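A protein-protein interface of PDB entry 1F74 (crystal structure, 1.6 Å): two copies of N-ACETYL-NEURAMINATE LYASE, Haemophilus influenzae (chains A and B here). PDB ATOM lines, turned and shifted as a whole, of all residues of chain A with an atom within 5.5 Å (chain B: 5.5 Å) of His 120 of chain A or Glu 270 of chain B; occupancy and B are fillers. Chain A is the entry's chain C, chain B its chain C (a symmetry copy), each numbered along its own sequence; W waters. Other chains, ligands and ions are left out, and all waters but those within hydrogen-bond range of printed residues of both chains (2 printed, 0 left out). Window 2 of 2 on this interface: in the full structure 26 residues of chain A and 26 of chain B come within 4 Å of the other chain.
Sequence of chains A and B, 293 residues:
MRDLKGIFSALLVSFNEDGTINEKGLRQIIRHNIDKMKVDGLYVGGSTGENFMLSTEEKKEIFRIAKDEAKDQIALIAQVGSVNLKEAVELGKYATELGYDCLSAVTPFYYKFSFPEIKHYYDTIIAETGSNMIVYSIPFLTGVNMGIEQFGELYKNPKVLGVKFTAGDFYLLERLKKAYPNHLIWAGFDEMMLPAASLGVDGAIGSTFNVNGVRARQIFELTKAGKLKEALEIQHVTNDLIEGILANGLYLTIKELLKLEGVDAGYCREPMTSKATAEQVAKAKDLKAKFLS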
ATOM      1  N   VAL A  83      26.776 -15.173   7.720  1.00  0.00           N
ATOM      2  CA  VAL A  83      27.372 -15.158   9.060  1.00  0.00           C
ATOM      3  C   VAL A  83      26.286 -15.505  10.076  1.00  0.00           C
ATOM      4  O   VAL A  83      26.570 -15.986  11.170  1.00  0.00           O
ATOM      5  CB  VAL A  83      27.990 -13.794   9.367  1.00  0.00           C
ATOM      6  CG1 VAL A  83      28.687 -13.790  10.718  1.00  0.00           C
ATOM      7  CG2 VAL A  83      28.985 -13.388   8.277  1.00  0.00           C
ATOM      8  N   LEU A  85      23.651 -17.971  11.008  1.00  0.00           N
ATOM      9  CA  LEU A  85      23.228 -19.355  10.714  1.00  0.00           C
ATOM     10  C   LEU A  85      21.719 -19.481  10.698  1.00  0.00           C
ATOM     11  O   LEU A  85      21.166 -20.269   9.909  1.00  0.00           O
ATOM     12  CB  LEU A  85      23.860 -20.315  11.715  1.00  0.00           C
ATOM     13  CG  LEU A  85      23.452 -21.795  11.632  1.00  0.00           C
ATOM     14  CD1 LEU A  85      23.756 -22.370  10.266  1.00  0.00           C
ATOM     15  CD2 LEU A  85      24.225 -22.571  12.708  1.00  0.00           C
ATOM     16  N   PHE A 115      37.423 -25.094  12.770  1.00  0.00           N
ATOM     17  CA  PHE A 115      36.894 -26.113  11.862  1.00  0.00           C
ATOM     18  C   PHE A 115      35.643 -26.752  12.416  1.00  0.00           C
ATOM     19  O   PHE A 115      34.600 -26.762  11.739  1.00  0.00           O
ATOM     20  CB  PHE A 115      37.957 -27.133  11.409  1.00  0.00           C
ATOM     21  CG  PHE A 115      37.261 -28.163  10.540  1.00  0.00           C
ATOM     22  CD1 PHE A 115      36.896 -27.826   9.247  1.00  0.00           C
ATOM     23  CD2 PHE A 115      36.942 -29.402  11.057  1.00  0.00           C
ATOM     24  CE1 PHE A 115      36.223 -28.757   8.462  1.00  0.00           C
ATOM     25  CE2 PHE A 115      36.268 -30.327  10.282  1.00  0.00           C
ATOM     26  CZ  PHE A 115      35.918 -29.996   8.988  1.00  0.00           C
ATOM     27  N   PRO A 116      35.569 -27.198  13.656  1.00  0.00           N
ATOM     28  CA  PRO A 116      34.351 -27.764  14.214  1.00  0.00           C
ATOM     29  C   PRO A 116      33.154 -26.842  14.032  1.00  0.00           C
ATOM     30  O   PRO A 116      32.033 -27.330  13.824  1.00  0.00           O
ATOM     31  CB  PRO A 116      34.724 -28.064  15.664  1.00  0.00           C
ATOM     32  CG  PRO A 116      36.199 -28.317  15.600  1.00  0.00           C
ATOM     33  CD  PRO A 116      36.710 -27.295  14.606  1.00  0.00           C
ATOM     34  N   GLU A 117      33.329 -25.532  14.188  1.00  0.00           N
ATOM     35  CA  GLU A 117      32.242 -24.576  14.009  1.00  0.00           C
ATOM     36  C   GLU A 117      31.775 -24.549  12.558  1.00  0.00           C
ATOM     37  O   GLU A 117      30.566 -24.514  12.322  1.00  0.00           O
ATOM     38  CB  GLU A 117      32.674 -23.173  14.473  1.00  0.00           C
ATOM     39  CG  GLU A 117      32.714 -23.094  15.999  1.00  0.00           C
ATOM     40  CD  GLU A 117      33.438 -21.862  16.501  1.00  0.00           C
ATOM     41  OE1 GLU A 117      34.068 -21.154  15.694  1.00  0.00           O
ATOM     42  OE2 GLU A 117      33.408 -21.583  17.726  1.00  0.00           O
ATOM     43  N   ILE A 118      32.697 -24.620  11.613  1.00  0.00           N
ATOM     44  CA  ILE A 118      32.343 -24.643  10.195  1.00  0.00           C
ATOM     45  C   ILE A 118      31.581 -25.925   9.861  1.00  0.00           C
ATOM     46  O   ILE A 118      30.570 -25.867   9.155  1.00  0.00           O
ATOM     47  CB  ILE A 118      33.599 -24.509   9.322  1.00  0.00           C
ATOM     48  CG1 ILE A 118      34.232 -23.125   9.524  1.00  0.00           C
ATOM     49  CG2 ILE A 118      33.271 -24.682   7.840  1.00  0.00           C
ATOM     50  CD1 ILE A 118      35.609 -22.948   8.928  1.00  0.00           C
ATOM     51  N   LYS A 119      32.052 -27.068  10.362  1.00  0.00           N
ATOM     52  CA  LYS A 119      31.343 -28.323  10.085  1.00  0.00           C
ATOM     53  C   LYS A 119      29.953 -28.299  10.703  1.00  0.00           C
ATOM     54  O   LYS A 119      28.984 -28.718  10.060  1.00  0.00           O
ATOM     55  CB  LYS A 119      32.145 -29.536  10.550  1.00  0.00           C
ATOM     56  CG  LYS A 119      31.375 -30.848  10.471  1.00  0.00           C
ATOM     57  CD  LYS A 119      32.340 -32.021  10.588  1.00  0.00           C
ATOM     58  CE  LYS A 119      31.584 -33.291  10.962  1.00  0.00           C
ATOM     59  NZ  LYS A 119      30.560 -33.650   9.944  1.00  0.00           N
ATOM     60  N   HIS A 120      29.822 -27.780  11.933  1.00  0.00           N
ATOM     61  CA  HIS A 120      28.501 -27.713  12.559  1.00  0.00           C
ATOM     62  C   HIS A 120      27.561 -26.808  11.770  1.00  0.00           C
ATOM     63  O   HIS A 120      26.364 -27.079  11.672  1.00  0.00           O
ATOM     64  CB  HIS A 120      28.649 -27.230  14.004  1.00  0.00           C
ATOM     65  CG  HIS A 120      27.335 -27.072  14.710  1.00  0.00           C
ATOM     66  ND1 HIS A 120      26.720 -25.852  14.869  1.00  0.00           N
ATOM     67  CD2 HIS A 120      26.529 -27.996  15.282  1.00  0.00           C
ATOM     68  CE1 HIS A 120      25.575 -26.045  15.509  1.00  0.00           C
ATOM     69  NE2 HIS A 120      25.442 -27.319  15.794  1.00  0.00           N
ATOM     70  N   TYR A 121      28.094 -25.721  11.206  1.00  0.00           N
ATOM     71  CA  TYR A 121      27.316 -24.806  10.366  1.00  0.00           C
ATOM     72  C   TYR A 121      26.732 -25.555   9.172  1.00  0.00           C
ATOM     73  O   TYR A 121      25.526 -25.523   8.923  1.00  0.00           O
ATOM     74  CB  TYR A 121      28.216 -23.660   9.931  1.00  0.00           C
ATOM     75  CG  TYR A 121      27.921 -22.749   8.788  1.00  0.00           C
ATOM     76  CD1 TYR A 121      28.277 -23.090   7.488  1.00  0.00           C
ATOM     77  CD2 TYR A 121      27.324 -21.488   8.981  1.00  0.00           C
ATOM     78  CE1 TYR A 121      28.055 -22.247   6.409  1.00  0.00           C
ATOM     79  CE2 TYR A 121      27.091 -20.647   7.907  1.00  0.00           C
ATOM     80  CZ  TYR A 121      27.456 -21.021   6.631  1.00  0.00           C
ATOM     81  OH  TYR A 121      27.259 -20.162   5.580  1.00  0.00           O
ATOM     82  N   TYR A 122      27.592 -26.291   8.445  1.00  0.00           N
ATOM     83  CA  TYR A 122      27.102 -27.050   7.302  1.00  0.00           C
ATOM     84  C   TYR A 122      26.146 -28.156   7.726  1.00  0.00           C
ATOM     85  O   TYR A 122      25.083 -28.304   7.106  1.00  0.00           O
ATOM     86  CB  TYR A 122      28.266 -27.688   6.524  1.00  0.00           C
ATOM     87  CG  TYR A 122      29.012 -26.696   5.652  1.00  0.00           C
ATOM     88  CD1 TYR A 122      28.390 -26.013   4.615  1.00  0.00           C
ATOM     89  CD2 TYR A 122      30.370 -26.491   5.866  1.00  0.00           C
ATOM     90  CE1 TYR A 122      29.094 -25.120   3.819  1.00  0.00           C
ATOM     91  CE2 TYR A 122      31.077 -25.596   5.086  1.00  0.00           C
ATOM     92  CZ  TYR A 122      30.440 -24.914   4.068  1.00  0.00           C
ATOM     93  OH  TYR A 122      31.159 -24.031   3.294  1.00  0.00           O
ATOM     94  N   ASP A 123      26.478 -28.901   8.773  1.00  0.00           N
ATOM     95  CA  ASP A 123      25.587 -29.988   9.202  1.00  0.00           C
ATOM     96  C   ASP A 123      24.232 -29.446   9.635  1.00  0.00           C
ATOM     97  O   ASP A 123      23.211 -30.113   9.436  1.00  0.00           O
ATOM     98  CB  ASP A 123      26.215 -30.808  10.326  1.00  0.00           C
ATOM     99  CG  ASP A 123      27.375 -31.669   9.858  1.00  0.00           C
ATOM    100  OD1 ASP A 123      27.443 -31.990   8.661  1.00  0.00           O
ATOM    101  OD2 ASP A 123      28.208 -31.995  10.723  1.00  0.00           O
ATOM    102  N   THR A 124      24.194 -28.260  10.245  1.00  0.00           N
ATOM    103  CA  THR A 124      22.933 -27.662  10.680  1.00  0.00           C
ATOM    104  C   THR A 124      22.074 -27.250   9.503  1.00  0.00           C
ATOM    105  O   THR A 124      20.877 -27.542   9.451  1.00  0.00           O
ATOM    106  CB  THR A 124      23.215 -26.459  11.598  1.00  0.00           C
ATOM    107  OG1 THR A 124      23.872 -26.914  12.787  1.00  0.00           O
ATOM    108  CG2 THR A 124      21.914 -25.746  11.959  1.00  0.00           C
ATOM    109  N   ILE A 125      22.642 -26.594   8.495  1.00  0.00           N
ATOM    110  CA  ILE A 125      21.870 -26.214   7.310  1.00  0.00           C
ATOM    111  C   ILE A 125      21.309 -27.471   6.632  1.00  0.00           C
ATOM    112  O   ILE A 125      20.138 -27.480   6.245  1.00  0.00           O
ATOM    113  CB  ILE A 125      22.676 -25.384   6.311  1.00  0.00           C
ATOM    114  CG1 ILE A 125      23.188 -24.108   6.995  1.00  0.00           C
ATOM    115  CG2 ILE A 125      21.840 -25.018   5.086  1.00  0.00           C
ATOM    116  CD1 ILE A 125      24.301 -23.412   6.215  1.00  0.00           C
ATOM    117  N   MET B  53      26.265 -12.051  13.476  1.00  0.00           N
ATOM    118  CA  MET B  53      25.552 -13.318  13.385  1.00  0.00           C
ATOM    119  C   MET B  53      24.060 -13.107  13.617  1.00  0.00           C
ATOM    120  O   MET B  53      23.345 -14.114  13.690  1.00  0.00           O
ATOM    121  CB  MET B  53      26.108 -14.311  14.426  1.00  0.00           C
ATOM    122  CG  MET B  53      27.562 -14.692  14.132  1.00  0.00           C
ATOM    123  SD  MET B  53      28.232 -15.904  15.283  1.00  0.00           S
ATOM    124  CE  MET B  53      28.363 -14.885  16.770  1.00  0.00           C
ATOM    125  N   CYS B 268      26.853 -18.311  23.820  1.00  0.00           N
ATOM    126  CA  CYS B 268      27.280 -17.600  22.617  1.00  0.00           C
ATOM    127  C   CYS B 268      26.277 -17.952  21.523  1.00  0.00           C
ATOM    128  O   CYS B 268      25.454 -18.860  21.689  1.00  0.00           O
ATOM    129  CB  CYS B 268      28.710 -17.955  22.196  1.00  0.00           C
ATOM    130  SG  CYS B 268      29.944 -16.961  23.085  1.00  0.00           S
ATOM    131  N   ARG B 269      26.307 -17.215  20.432  1.00  0.00           N
ATOM    132  CA  ARG B 269      25.393 -17.393  19.316  1.00  0.00           C
ATOM    133  C   ARG B 269      26.051 -18.182  18.183  1.00  0.00           C
ATOM    134  O   ARG B 269      27.108 -17.824  17.697  1.00  0.00           O
ATOM    135  CB  ARG B 269      24.994 -16.000  18.823  1.00  0.00           C
ATOM    136  CG  ARG B 269      24.243 -15.975  17.514  1.00  0.00           C
ATOM    137  CD  ARG B 269      22.802 -16.452  17.693  1.00  0.00           C
ATOM    138  NE  ARG B 269      22.127 -16.249  16.422  1.00  0.00           N
ATOM    139  CZ  ARG B 269      21.015 -15.616  16.148  1.00  0.00           C
ATOM    140  NH1 ARG B 269      20.321 -15.064  17.134  1.00  0.00           N
ATOM    141  NH2 ARG B 269      20.657 -15.569  14.873  1.00  0.00           N
ATOM    142  N   GLU B 270      25.309 -19.190  17.715  1.00  0.00           N
ATOM    143  CA  GLU B 270      25.790 -20.013  16.621  1.00  0.00           C
ATOM    144  C   GLU B 270      25.800 -19.330  15.279  1.00  0.00           C
ATOM    145  O   GLU B 270      24.990 -18.417  15.411  1.00  0.00           O
ATOM    146  CB  GLU B 270      24.959 -21.304  16.487  1.00  0.00           C
ATOM    147  CG  GLU B 270      25.124 -22.278  17.633  1.00  0.00           C
ATOM    148  CD  GLU B 270      24.506 -23.640  17.403  1.00  0.00           C
ATOM    149  OE1 GLU B 270      23.663 -23.809  16.498  1.00  0.00           O
ATOM    150  OE2 GLU B 270      24.875 -24.565  18.166  1.00  0.00           O
ATOM    151  N   PRO B 271      26.923 -19.292  14.604  1.00  0.00           N
ATOM    152  CA  PRO B 271      27.803 -20.369  14.288  1.00  0.00           C
ATOM    153  C   PRO B 271      29.006 -20.423  15.233  1.00  0.00           C
ATOM    154  O   PRO B 271      29.828 -21.339  15.153  1.00  0.00           O
ATOM    155  CB  PRO B 271      28.217 -20.352  12.827  1.00  0.00           C
ATOM    156  CG  PRO B 271      28.076 -18.901  12.506  1.00  0.00           C
ATOM    157  CD  PRO B 271      26.906 -18.516  13.342  1.00  0.00           C
ATOM    158  N   MET B 272      29.091 -19.477  16.178  1.00  0.00           N
ATOM    159  CA  MET B 272      30.136 -19.631  17.196  1.00  0.00           C
ATOM    160  C   MET B 272      29.695 -20.761  18.130  1.00  0.00           C
ATOM    161  O   MET B 272      28.491 -20.960  18.321  1.00  0.00           O
ATOM    162  CB  MET B 272      30.361 -18.363  17.998  1.00  0.00           C
ATOM    163  CG  MET B 272      31.074 -17.247  17.250  1.00  0.00           C
ATOM    164  SD  MET B 272      31.874 -16.040  18.322  1.00  0.00           S
ATOM    165  CE  MET B 272      32.646 -14.997  17.087  1.00  0.00           C
ATOM    166  N   THR B 273      30.623 -21.518  18.709  1.00  0.00           N
ATOM    167  CA  THR B 273      30.273 -22.566  19.668  1.00  0.00           C
ATOM    168  C   THR B 273      29.411 -21.900  20.742  1.00  0.00           C
ATOM    169  O   THR B 273      29.885 -20.923  21.332  1.00  0.00           O
ATOM    170  CB  THR B 273      31.528 -23.180  20.294  1.00  0.00           C
ATOM    171  OG1 THR B 273      32.322 -23.759  19.239  1.00  0.00           O
ATOM    172  CG2 THR B 273      31.176 -24.260  21.303  1.00  0.00           C
ATOM    173  N   SER B 274      28.200 -22.394  20.960  1.00  0.00           N
ATOM    174  CA  SER B 274      27.305 -21.730  21.903  1.00  0.00           C
ATOM    175  C   SER B 274      27.550 -22.079  23.362  1.00  0.00           C
ATOM    176  O   SER B 274      27.400 -21.210  24.230  1.00  0.00           O
ATOM    177  CB  SER B 274      25.829 -22.003  21.559  1.00  0.00           C
ATOM    178  OG  SER B 274      25.554 -23.390  21.590  1.00  0.00           O
HETATM  179  O   HOH W   1      23.430 -16.897  13.719  1.00  0.00           O
HETATM  180  O   HOH W   2      28.698 -23.671  14.176  1.00  0.00           O
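Water W1 lies within hydrogen-bond range of O of Glu 270 of chain B, O of Met 53 of chain B, N of Leu 85 of chain A and NE of Arg 269 of chain B.
Water W2 lies within hydrogen-bond range of the backbone carbonyl oxygen (O) of Glu 117 of chain A (2.8 Å), the backbone carbonyl oxygen (O) of Pro 271 of chain B (2.8 Å) and a ring nitrogen (ND1) of His 120 of chain A (3.0 Å).
No position is printed for both chains.
Of the 7 pairs that touch across the chains among the printed residues, none has its exchanged pair printed and touching as well.
Printed residues of chain B within 4 Å of Leu 85 of chain A: Pro 271.
Phe 115 of chain A touches none of the printed residues of chain B.
Of the printed residues of chain B, His 120 of chain A touches Glu 270 (3.1 Å).
Of the printed residues of chain A, Glu 270 of chain B touches His 120 (3.1 Å).
Of the printed residues of chain A, Pro 271 of chain B touches Val 83, Leu 85 and Glu 117.
Printed residues of chain A within 4 Å of Met 272 of chain B: Glu 117 (3.8 Å).
The nearest printed residue of chain B that does not touch His 120 of chain A is Pro 271 of chain B (5.5 Å).
The nearest printed residue of chain A that does not touch Glu 270 of chain B is Leu 85 of chain A (4.03 Å).
Printed residues of chain A that touch a printed residue of chain B: Val 83, Leu 85, Glu 117 and His 120.
Hydrophobic or aromatic side chains of chain A that line the printed part of chain B: Val 83, Leu 85 and His 120.
Of the 8 printed residues of chain B, 5 touch a printed residue of chain A.
Hydrophobic or aromatic side chains of chain B that line the printed part of chain A: Met 53 and Pro 271.
Among the printed residues, no Asp or Glu carboxylate lies within 4 Å of a Lys or Arg side-chain nitrogen of the other chain.
The side-chain carboxylate (OE2) of Glu 117 of chain A is in hydrogen-bond range of the side-chain hydroxyl (OG1) of Thr 273 of chain B (2.9 Å).
The backbone NH of Met 272 of chain B sits close to the side-chain sulfur of Met 53 of chain B (3.8 Å).
The guanidinium group of Arg 269 of chain B lies within hydrogen-bond range of the backbone carbonyl oxygen of Met 53 of chain B (3.3 Å).
The side-chain hydroxyl (OG1) of Thr 124 of chain A lies within hydrogen-bond range of the backbone carbonyl oxygen (O) of His 120 of chain A (2.7 Å).
O of Val 83 of chain A touches CG of Met 53 of chain B (3.4 Å).
Pro 271 of chain B touches Val 83 of chain A (CD to O, 3.4 Å).
Leu 85 of chain A touches Pro 271 of chain B.
Pro 271 of chain B touches Glu 117 of chain A (O to CB, 3.5 Å).
Glu 117 of chain A touches Met 272 of chain B (OE2 to C, 3.8 Å).
CE1 of His 120 of chain A touches OE1 of Glu 270 of chain B, at 3.1 Å.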
